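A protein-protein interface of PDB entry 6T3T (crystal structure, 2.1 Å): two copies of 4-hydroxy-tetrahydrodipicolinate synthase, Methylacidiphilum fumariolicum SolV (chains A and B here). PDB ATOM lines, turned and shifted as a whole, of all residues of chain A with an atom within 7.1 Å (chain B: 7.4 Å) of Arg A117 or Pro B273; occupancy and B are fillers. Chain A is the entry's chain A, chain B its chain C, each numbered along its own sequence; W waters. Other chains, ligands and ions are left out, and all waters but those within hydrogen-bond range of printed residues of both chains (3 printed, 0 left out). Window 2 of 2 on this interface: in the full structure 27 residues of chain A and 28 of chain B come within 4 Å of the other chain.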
ATOM      1  N   THR A  82       9.642  21.580  27.543  1.00  0.00           N
ATOM      2  CA  THR A  82       8.550  21.144  26.670  1.00  0.00           C
ATOM      3  C   THR A  82       8.240  19.655  26.838  1.00  0.00           C
ATOM      4  O   THR A  82       7.070  19.261  26.955  1.00  0.00           O
ATOM      5  CB  THR A  82       8.902  21.447  25.214  1.00  0.00           C
ATOM      6  OG1 THR A  82       9.219  22.833  25.103  1.00  0.00           O
ATOM      7  CG2 THR A  82       7.694  21.106  24.282  1.00  0.00           C
ATOM      8  N   SER A 111      12.323  32.736  23.185  1.00  0.00           N
ATOM      9  CA  SER A 111      11.851  33.678  22.185  1.00  0.00           C
ATOM     10  C   SER A 111      10.387  33.363  21.838  1.00  0.00           C
ATOM     11  O   SER A 111       9.852  32.310  22.205  1.00  0.00           O
ATOM     12  CB  SER A 111      12.726  33.582  20.941  1.00  0.00           C
ATOM     13  OG  SER A 111      12.549  32.295  20.378  1.00  0.00           O
ATOM     14  N   GLN A 112       9.737  34.293  21.124  1.00  0.00           N
ATOM     15  CA  GLN A 112       8.343  34.094  20.723  1.00  0.00           C
ATOM     16  C   GLN A 112       8.184  32.855  19.871  1.00  0.00           C
ATOM     17  O   GLN A 112       7.201  32.111  19.996  1.00  0.00           O
ATOM     18  CB  GLN A 112       7.819  35.307  19.948  1.00  0.00           C
ATOM     19  CG  GLN A 112       7.590  36.528  20.792  1.00  0.00           C
ATOM     20  CD  GLN A 112       6.755  36.209  22.010  1.00  0.00           C
ATOM     21  OE1 GLN A 112       5.628  35.711  21.911  1.00  0.00           O
ATOM     22  NE2 GLN A 112       7.332  36.444  23.176  1.00  0.00           N
ATOM     23  N   GLU A 113       9.129  32.625  18.977  1.00  0.00           N
ATOM     24  CA  GLU A 113       9.104  31.407  18.190  1.00  0.00           C
ATOM     25  C   GLU A 113       9.293  30.182  19.081  1.00  0.00           C
ATOM     26  O   GLU A 113       8.638  29.148  18.884  1.00  0.00           O
ATOM     27  CB  GLU A 113      10.185  31.511  17.111  1.00  0.00           C
ATOM     28  CG  GLU A 113       9.825  30.961  15.808  1.00  0.00           C
ATOM     29  CD  GLU A 113       8.392  31.265  15.391  1.00  0.00           C
ATOM     30  OE1 GLU A 113       7.963  32.428  15.349  1.00  0.00           O
ATOM     31  OE2 GLU A 113       7.659  30.294  15.155  1.00  0.00           O
ATOM     32  N   GLY A 114      10.171  30.290  20.075  1.00  0.00           N
ATOM     33  CA  GLY A 114      10.284  29.227  21.059  1.00  0.00           C
ATOM     34  C   GLY A 114       8.973  28.949  21.774  1.00  0.00           C
ATOM     35  O   GLY A 114       8.586  27.792  21.932  1.00  0.00           O
ATOM     36  N   LEU A 115       8.257  30.012  22.196  1.00  0.00           N
ATOM     37  CA  LEU A 115       6.952  29.835  22.827  1.00  0.00           C
ATOM     38  C   LEU A 115       5.962  29.183  21.862  1.00  0.00           C
ATOM     39  O   LEU A 115       5.219  28.269  22.248  1.00  0.00           O
ATOM     40  CB  LEU A 115       6.402  31.187  23.303  1.00  0.00           C
ATOM     41  CG  LEU A 115       7.101  31.877  24.472  1.00  0.00           C
ATOM     42  CD1 LEU A 115       6.404  33.179  24.825  1.00  0.00           C
ATOM     43  CD2 LEU A 115       7.140  30.966  25.698  1.00  0.00           C
ATOM     44  N   PHE A 116       5.968  29.615  20.592  1.00  0.00           N
ATOM     45  CA  PHE A 116       5.100  28.998  19.585  1.00  0.00           C
ATOM     46  C   PHE A 116       5.352  27.488  19.477  1.00  0.00           C
ATOM     47  O   PHE A 116       4.418  26.681  19.494  1.00  0.00           O
ATOM     48  CB  PHE A 116       5.294  29.660  18.209  1.00  0.00           C
ATOM     49  CG  PHE A 116       4.561  28.931  17.107  1.00  0.00           C
ATOM     50  CD1 PHE A 116       3.200  29.129  16.919  1.00  0.00           C
ATOM     51  CD2 PHE A 116       5.205  27.978  16.318  1.00  0.00           C
ATOM     52  CE1 PHE A 116       2.504  28.421  15.922  1.00  0.00           C
ATOM     53  CE2 PHE A 116       4.505  27.268  15.327  1.00  0.00           C
ATOM     54  CZ  PHE A 116       3.158  27.497  15.134  1.00  0.00           C
ATOM     55  N   ARG A 117       6.616  27.088  19.376  1.00  0.00           N
ATOM     56  CA  ARG A 117       6.915  25.665  19.236  1.00  0.00           C
ATOM     57  C   ARG A 117       6.647  24.899  20.517  1.00  0.00           C
ATOM     58  O   ARG A 117       6.198  23.755  20.465  1.00  0.00           O
ATOM     59  CB  ARG A 117       8.348  25.486  18.786  1.00  0.00           C
ATOM     60  CG  ARG A 117       8.435  25.804  17.322  1.00  0.00           C
ATOM     61  CD  ARG A 117       9.848  25.721  16.835  1.00  0.00           C
ATOM     62  NE  ARG A 117      10.334  24.353  16.903  1.00  0.00           N
ATOM     63  CZ  ARG A 117      11.566  24.013  16.578  1.00  0.00           C
ATOM     64  NH1 ARG A 117      12.393  24.965  16.162  1.00  0.00           N
ATOM     65  NH2 ARG A 117      11.957  22.743  16.664  1.00  0.00           N
ATOM     66  N   HIS A 118       6.906  25.516  21.670  1.00  0.00           N
ATOM     67  CA  HIS A 118       6.648  24.869  22.953  1.00  0.00           C
ATOM     68  C   HIS A 118       5.176  24.507  23.075  1.00  0.00           C
ATOM     69  O   HIS A 118       4.813  23.333  23.253  1.00  0.00           O
ATOM     70  CB  HIS A 118       7.084  25.797  24.098  1.00  0.00           C
ATOM     71  CG  HIS A 118       6.622  25.370  25.460  1.00  0.00           C
ATOM     72  ND1 HIS A 118       7.280  24.417  26.210  1.00  0.00           N
ATOM     73  CD2 HIS A 118       5.576  25.784  26.215  1.00  0.00           C
ATOM     74  CE1 HIS A 118       6.670  24.273  27.374  1.00  0.00           C
ATOM     75  NE2 HIS A 118       5.628  25.083  27.395  1.00  0.00           N
ATOM     76  N   PHE A 119       4.309  25.515  22.957  1.00  0.00           N
ATOM     77  CA  PHE A 119       2.885  25.291  23.114  1.00  0.00           C
ATOM     78  C   PHE A 119       2.318  24.445  21.972  1.00  0.00           C
ATOM     79  O   PHE A 119       1.416  23.629  22.205  1.00  0.00           O
ATOM     80  CB  PHE A 119       2.165  26.633  23.204  1.00  0.00           C
ATOM     81  CG  PHE A 119       2.405  27.383  24.503  1.00  0.00           C
ATOM     82  CD1 PHE A 119       2.079  26.802  25.732  1.00  0.00           C
ATOM     83  CD2 PHE A 119       2.896  28.675  24.487  1.00  0.00           C
ATOM     84  CE1 PHE A 119       2.275  27.482  26.939  1.00  0.00           C
ATOM     85  CE2 PHE A 119       3.095  29.388  25.688  1.00  0.00           C
ATOM     86  CZ  PHE A 119       2.766  28.782  26.926  1.00  0.00           C
ATOM     87  N   SER A 120       2.834  24.613  20.747  1.00  0.00           N
ATOM     88  CA  SER A 120       2.375  23.788  19.622  1.00  0.00           C
ATOM     89  C   SER A 120       2.708  22.318  19.830  1.00  0.00           C
ATOM     90  O   SER A 120       1.916  21.446  19.465  1.00  0.00           O
ATOM     91  CB  SER A 120       2.964  24.279  18.300  1.00  0.00           C
ATOM     92  OG  SER A 120       2.397  25.519  17.909  1.00  0.00           O
ATOM     93  N   ALA A 121       3.905  22.016  20.356  1.00  0.00           N
ATOM     94  CA  ALA A 121       4.263  20.615  20.564  1.00  0.00           C
ATOM     95  C   ALA A 121       3.363  19.963  21.608  1.00  0.00           C
ATOM     96  O   ALA A 121       2.953  18.811  21.448  1.00  0.00           O
ATOM     97  CB  ALA A 121       5.742  20.488  20.949  1.00  0.00           C
ATOM     98  N   ILE A 122       3.033  20.679  22.682  1.00  0.00           N
ATOM     99  CA  ILE A 122       2.152  20.094  23.687  1.00  0.00           C
ATOM    100  C   ILE A 122       0.763  19.902  23.102  1.00  0.00           C
ATOM    101  O   ILE A 122       0.173  18.820  23.220  1.00  0.00           O
ATOM    102  CB  ILE A 122       2.116  20.973  24.958  1.00  0.00           C
ATOM    103  CG1 ILE A 122       3.530  21.300  25.461  1.00  0.00           C
ATOM    104  CG2 ILE A 122       1.296  20.313  26.046  1.00  0.00           C
ATOM    105  CD1 ILE A 122       3.640  22.669  26.189  1.00  0.00           C
ATOM    106  N   ALA A 123       0.244  20.922  22.396  1.00  0.00           N
ATOM    107  CA  ALA A 123      -1.090  20.799  21.803  1.00  0.00           C
ATOM    108  C   ALA A 123      -1.171  19.618  20.843  1.00  0.00           C
ATOM    109  O   ALA A 123      -2.139  18.855  20.871  1.00  0.00           O
ATOM    110  CB  ALA A 123      -1.491  22.085  21.089  1.00  0.00           C
ATOM    111  N   THR A 147       1.739  35.894  18.839  1.00  0.00           N
ATOM    112  CA  THR A 147       2.039  34.496  19.133  1.00  0.00           C
ATOM    113  C   THR A 147       0.775  33.744  19.552  1.00  0.00           C
ATOM    114  O   THR A 147       0.511  32.648  19.050  1.00  0.00           O
ATOM    115  CB  THR A 147       3.104  34.390  20.220  1.00  0.00           C
ATOM    116  OG1 THR A 147       4.224  35.216  19.883  1.00  0.00           O
ATOM    117  CG2 THR A 147       3.559  32.933  20.412  1.00  0.00           C
ATOM    118  N   LEU A 151      -0.773  30.583  17.491  1.00  0.00           N
ATOM    119  CA  LEU A 151      -1.039  29.335  18.205  1.00  0.00           C
ATOM    120  C   LEU A 151      -2.455  28.856  17.949  1.00  0.00           C
ATOM    121  O   LEU A 151      -2.677  27.685  17.634  1.00  0.00           O
ATOM    122  CB  LEU A 151      -0.813  29.534  19.717  1.00  0.00           C
ATOM    123  CG  LEU A 151       0.688  29.607  20.023  1.00  0.00           C
ATOM    124  CD1 LEU A 151       0.959  30.037  21.417  1.00  0.00           C
ATOM    125  CD2 LEU A 151       1.293  28.227  19.757  1.00  0.00           C
ATOM    126  N   GLU B 247      19.116  37.242  21.425  1.00  0.00           N
ATOM    127  CA  GLU B 247      17.971  36.508  21.960  1.00  0.00           C
ATOM    128  C   GLU B 247      18.446  35.785  23.235  1.00  0.00           C
ATOM    129  O   GLU B 247      19.615  35.890  23.634  1.00  0.00           O
ATOM    130  CB  GLU B 247      17.370  35.546  20.912  1.00  0.00           C
ATOM    131  CG  GLU B 247      17.012  36.224  19.576  1.00  0.00           C
ATOM    132  CD  GLU B 247      16.313  35.303  18.532  1.00  0.00           C
ATOM    133  OE1 GLU B 247      15.731  34.249  18.900  1.00  0.00           O
ATOM    134  OE2 GLU B 247      16.392  35.635  17.320  1.00  0.00           O
ATOM    135  N   VAL B 251      21.034  30.594  23.400  1.00  0.00           N
ATOM    136  CA  VAL B 251      20.885  30.395  21.953  1.00  0.00           C
ATOM    137  C   VAL B 251      21.994  31.095  21.170  1.00  0.00           C
ATOM    138  O   VAL B 251      22.608  30.447  20.306  1.00  0.00           O
ATOM    139  CB  VAL B 251      19.474  30.792  21.488  1.00  0.00           C
ATOM    140  CG1 VAL B 251      19.343  30.613  19.953  1.00  0.00           C
ATOM    141  CG2 VAL B 251      18.394  29.965  22.204  1.00  0.00           C
ATOM    142  N   THR B 255      24.708  28.828  19.157  1.00  0.00           N
ATOM    143  CA  THR B 255      24.735  29.059  17.719  1.00  0.00           C
ATOM    144  C   THR B 255      26.128  29.476  17.282  1.00  0.00           C
ATOM    145  O   THR B 255      26.642  28.984  16.271  1.00  0.00           O
ATOM    146  CB  THR B 255      23.709  30.142  17.337  1.00  0.00           C
ATOM    147  OG1 THR B 255      22.410  29.757  17.790  1.00  0.00           O
ATOM    148  CG2 THR B 255      23.648  30.328  15.858  1.00  0.00           C
ATOM    149  N   LEU B 265      24.260  22.517  16.478  1.00  0.00           N
ATOM    150  CA  LEU B 265      23.218  23.482  16.827  1.00  0.00           C
ATOM    151  C   LEU B 265      21.963  22.690  17.220  1.00  0.00           C
ATOM    152  O   LEU B 265      20.963  22.630  16.503  1.00  0.00           O
ATOM    153  CB  LEU B 265      22.936  24.429  15.670  1.00  0.00           C
ATOM    154  CG  LEU B 265      22.592  25.890  16.022  1.00  0.00           C
ATOM    155  CD1 LEU B 265      22.491  26.734  14.765  1.00  0.00           C
ATOM    156  CD2 LEU B 265      21.308  26.005  16.804  1.00  0.00           C
ATOM    157  N   LEU B 267      19.312  22.533  20.283  1.00  0.00           N
ATOM    158  CA  LEU B 267      18.647  23.143  21.420  1.00  0.00           C
ATOM    159  C   LEU B 267      17.479  22.265  21.857  1.00  0.00           C
ATOM    160  O   LEU B 267      16.930  21.500  21.058  1.00  0.00           O
ATOM    161  CB  LEU B 267      18.139  24.532  21.020  1.00  0.00           C
ATOM    162  CG  LEU B 267      19.284  25.462  20.622  1.00  0.00           C
ATOM    163  CD1 LEU B 267      18.776  26.671  19.870  1.00  0.00           C
ATOM    164  CD2 LEU B 267      19.971  25.910  21.890  1.00  0.00           C
ATOM    165  N   LEU B 269      13.613  22.274  23.162  1.00  0.00           N
ATOM    166  CA  LEU B 269      12.433  23.103  23.349  1.00  0.00           C
ATOM    167  C   LEU B 269      12.180  23.302  24.845  1.00  0.00           C
ATOM    168  O   LEU B 269      12.225  22.334  25.620  1.00  0.00           O
ATOM    169  CB  LEU B 269      11.204  22.454  22.677  1.00  0.00           C
ATOM    170  CG  LEU B 269      11.172  22.505  21.136  1.00  0.00           C
ATOM    171  CD1 LEU B 269       9.898  21.878  20.576  1.00  0.00           C
ATOM    172  CD2 LEU B 269      11.341  23.961  20.597  1.00  0.00           C
ATOM    173  N   PRO B 270      11.808  24.511  25.282  1.00  0.00           N
ATOM    174  CA  PRO B 270      11.306  25.612  24.455  1.00  0.00           C
ATOM    175  C   PRO B 270      12.324  26.546  23.803  1.00  0.00           C
ATOM    176  O   PRO B 270      11.858  27.454  23.112  1.00  0.00           O
ATOM    177  CB  PRO B 270      10.462  26.410  25.453  1.00  0.00           C
ATOM    178  CG  PRO B 270      11.218  26.285  26.734  1.00  0.00           C
ATOM    179  CD  PRO B 270      11.802  24.862  26.714  1.00  0.00           C
ATOM    180  N   LEU B 271      13.636  26.373  23.951  1.00  0.00           N
ATOM    181  CA  LEU B 271      14.519  27.250  23.187  1.00  0.00           C
ATOM    182  C   LEU B 271      14.454  26.876  21.705  1.00  0.00           C
ATOM    183  O   LEU B 271      14.257  25.711  21.350  1.00  0.00           O
ATOM    184  CB  LEU B 271      15.963  27.180  23.695  1.00  0.00           C
ATOM    185  CG  LEU B 271      16.148  27.605  25.155  1.00  0.00           C
ATOM    186  CD1 LEU B 271      17.596  27.698  25.522  1.00  0.00           C
ATOM    187  CD2 LEU B 271      15.417  28.922  25.453  1.00  0.00           C
ATOM    188  N   ALA B 272      14.567  27.881  20.844  1.00  0.00           N
ATOM    189  CA  ALA B 272      14.517  27.725  19.396  1.00  0.00           C
ATOM    190  C   ALA B 272      15.649  28.525  18.777  1.00  0.00           C
ATOM    191  O   ALA B 272      16.165  29.453  19.401  1.00  0.00           O
ATOM    192  CB  ALA B 272      13.184  28.203  18.802  1.00  0.00           C
ATOM    193  N   PRO B 273      16.073  28.183  17.560  1.00  0.00           N
ATOM    194  CA  PRO B 273      17.169  28.933  16.933  1.00  0.00           C
ATOM    195  C   PRO B 273      16.835  30.405  16.694  1.00  0.00           C
ATOM    196  O   PRO B 273      15.673  30.826  16.658  1.00  0.00           O
ATOM    197  CB  PRO B 273      17.390  28.199  15.602  1.00  0.00           C
ATOM    198  CG  PRO B 273      16.897  26.805  15.846  1.00  0.00           C
ATOM    199  CD  PRO B 273      15.720  26.969  16.803  1.00  0.00           C
ATOM    200  N   LEU B 274      17.895  31.187  16.492  1.00  0.00           N
ATOM    201  CA  LEU B 274      17.755  32.618  16.269  1.00  0.00           C
ATOM    202  C   LEU B 274      16.899  32.886  15.041  1.00  0.00           C
ATOM    203  O   LEU B 274      16.963  32.164  14.046  1.00  0.00           O
ATOM    204  CB  LEU B 274      19.123  33.254  16.043  1.00  0.00           C
ATOM    205  CG  LEU B 274      20.163  33.136  17.154  1.00  0.00           C
ATOM    206  CD1 LEU B 274      21.472  33.814  16.697  1.00  0.00           C
ATOM    207  CD2 LEU B 274      19.613  33.763  18.427  1.00  0.00           C
ATOM    208  N   GLN B 275      16.119  33.957  15.102  1.00  0.00           N
ATOM    209  CA  GLN B 275      15.466  34.451  13.898  1.00  0.00           C
ATOM    210  C   GLN B 275      16.514  34.931  12.888  1.00  0.00           C
ATOM    211  O   GLN B 275      17.627  35.313  13.262  1.00  0.00           O
ATOM    212  CB  GLN B 275      14.439  35.522  14.252  1.00  0.00           C
ATOM    213  CG  GLN B 275      13.201  34.790  14.825  1.00  0.00           C
ATOM    214  CD  GLN B 275      12.027  34.719  13.841  1.00  0.00           C
ATOM    215  OE1 GLN B 275      11.094  35.511  13.899  1.00  0.00           O
ATOM    216  NE2 GLN B 275      12.121  33.820  12.892  1.00  0.00           N
ATOM    217  N   PRO B 276      16.217  34.820  11.587  1.00  0.00           N
ATOM    218  CA  PRO B 276      17.292  34.952  10.578  1.00  0.00           C
ATOM    219  C   PRO B 276      18.084  36.249  10.635  1.00  0.00           C
ATOM    220  O   PRO B 276      19.317  36.202  10.488  1.00  0.00           O
ATOM    221  CB  PRO B 276      16.537  34.829   9.253  1.00  0.00           C
ATOM    222  CG  PRO B 276      15.300  34.033   9.592  1.00  0.00           C
ATOM    223  CD  PRO B 276      14.924  34.437  10.986  1.00  0.00           C
ATOM    224  N   LEU B 279      20.477  36.033  13.428  1.00  0.00           N
ATOM    225  CA  LEU B 279      21.566  35.136  13.057  1.00  0.00           C
ATOM    226  C   LEU B 279      22.642  35.880  12.273  1.00  0.00           C
ATOM    227  O   LEU B 279      23.836  35.709  12.536  1.00  0.00           O
ATOM    228  CB  LEU B 279      21.042  33.948  12.246  1.00  0.00           C
ATOM    229  CG  LEU B 279      22.130  32.930  11.881  1.00  0.00           C
ATOM    230  CD1 LEU B 279      22.601  32.294  13.160  1.00  0.00           C
ATOM    231  CD2 LEU B 279      21.683  31.875  10.873  1.00  0.00           C
HETATM  232  O   HOH W   1      12.097  19.666  26.115  1.00  0.00           O
HETATM  233  O   HOH W   2      14.292  30.574  21.994  1.00  0.00           O
HETATM  234  O   HOH W   3      13.785  32.933  17.800  1.00  0.00           O
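A ring nitrogen (ND1) of His A118 is in hydrogen-bond range of the side-chain hydroxyl of Thr A82 (2.7 Å).
OG of Ser A111 sits at hydrogen-bond distance from N of Gly A114, 3.1 Å away.
OE2 of Glu B247 is in hydrogen-bond range of N of Gln B275.
The side-chain hydroxyl (OG1) of Thr A82 lies close to the backbone carbonyl oxygen (O) of Leu B269, 3.1 Å away.
OG1 of Thr A82 lies close to N of Pro B270 (3.1 Å).
The backbone carbonyl oxygen (O) of Pro B270 lies close to the backbone carbonyl oxygen (O) of Gly A114 (3.5 Å).
Water W3 lies within hydrogen-bond range of OE1 of Glu B247, OG of Ser A111 and O of Pro B273.
Water W1 bridges the backbone carbonyl oxygen of Leu B269 and the backbone NH of Thr A82.
Water W2 lies within hydrogen-bond range of OG of Ser A111 (2.9 Å) and N of Ala B272 (2.9 Å).
Ser A111 touches Glu B247 (CB to OE1, 3.7 Å).
CB of Ala B272 touches CA of Gly A114, 3.8 Å away.
Leu B269 touches Arg A117 (CD2 to CB, 3.8 Å).
Arg A117 touches Pro B273 (NH1 to CD, 3.9 Å).
His A118 touches Pro B270 (CB to CB, 3.7 Å).
Of the printed residues of chain B, Arg A117 touches Leu B269 (3.8 Å) and Pro B273 (3.9 Å).
Pro B273 touches just one residue of chain A: Arg A117 (3.9 Å).
Printed residues of chain B within 4 Å of Thr A82: Leu B269 (3.0 Å) and Pro B270 (3.1 Å).
Printed residues of chain B within 4 Å of Ser A111: Glu B247.
Of the printed residues of chain A, Glu B247 touches Ser A111.
Of the printed residues of chain B, Gly A114 touches Pro B270 and Ala B272.
Leu A115 touches none of the printed residues of chain B.
Ile A122 touches none of the printed residues of chain B.
The nearest residue of chain A that does not touch Pro B273 is Ser A111 (5.1 Å).
The nearest printed residue of chain A that does not touch Pro B270 is Leu A115 (4.5 Å).
Of the 14 printed residues of chain B, 5 touch a printed residue of chain A.
Hydrophobic or aromatic side chains of chain B within 4 Å of the printed part of chain A: Leu B269, Pro B270, Ala B272 and Pro B273.
No position is printed for both chains.
Of the 8 pairs that touch across the chains among the printed residues, none has its exchanged pair printed and touching as well.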
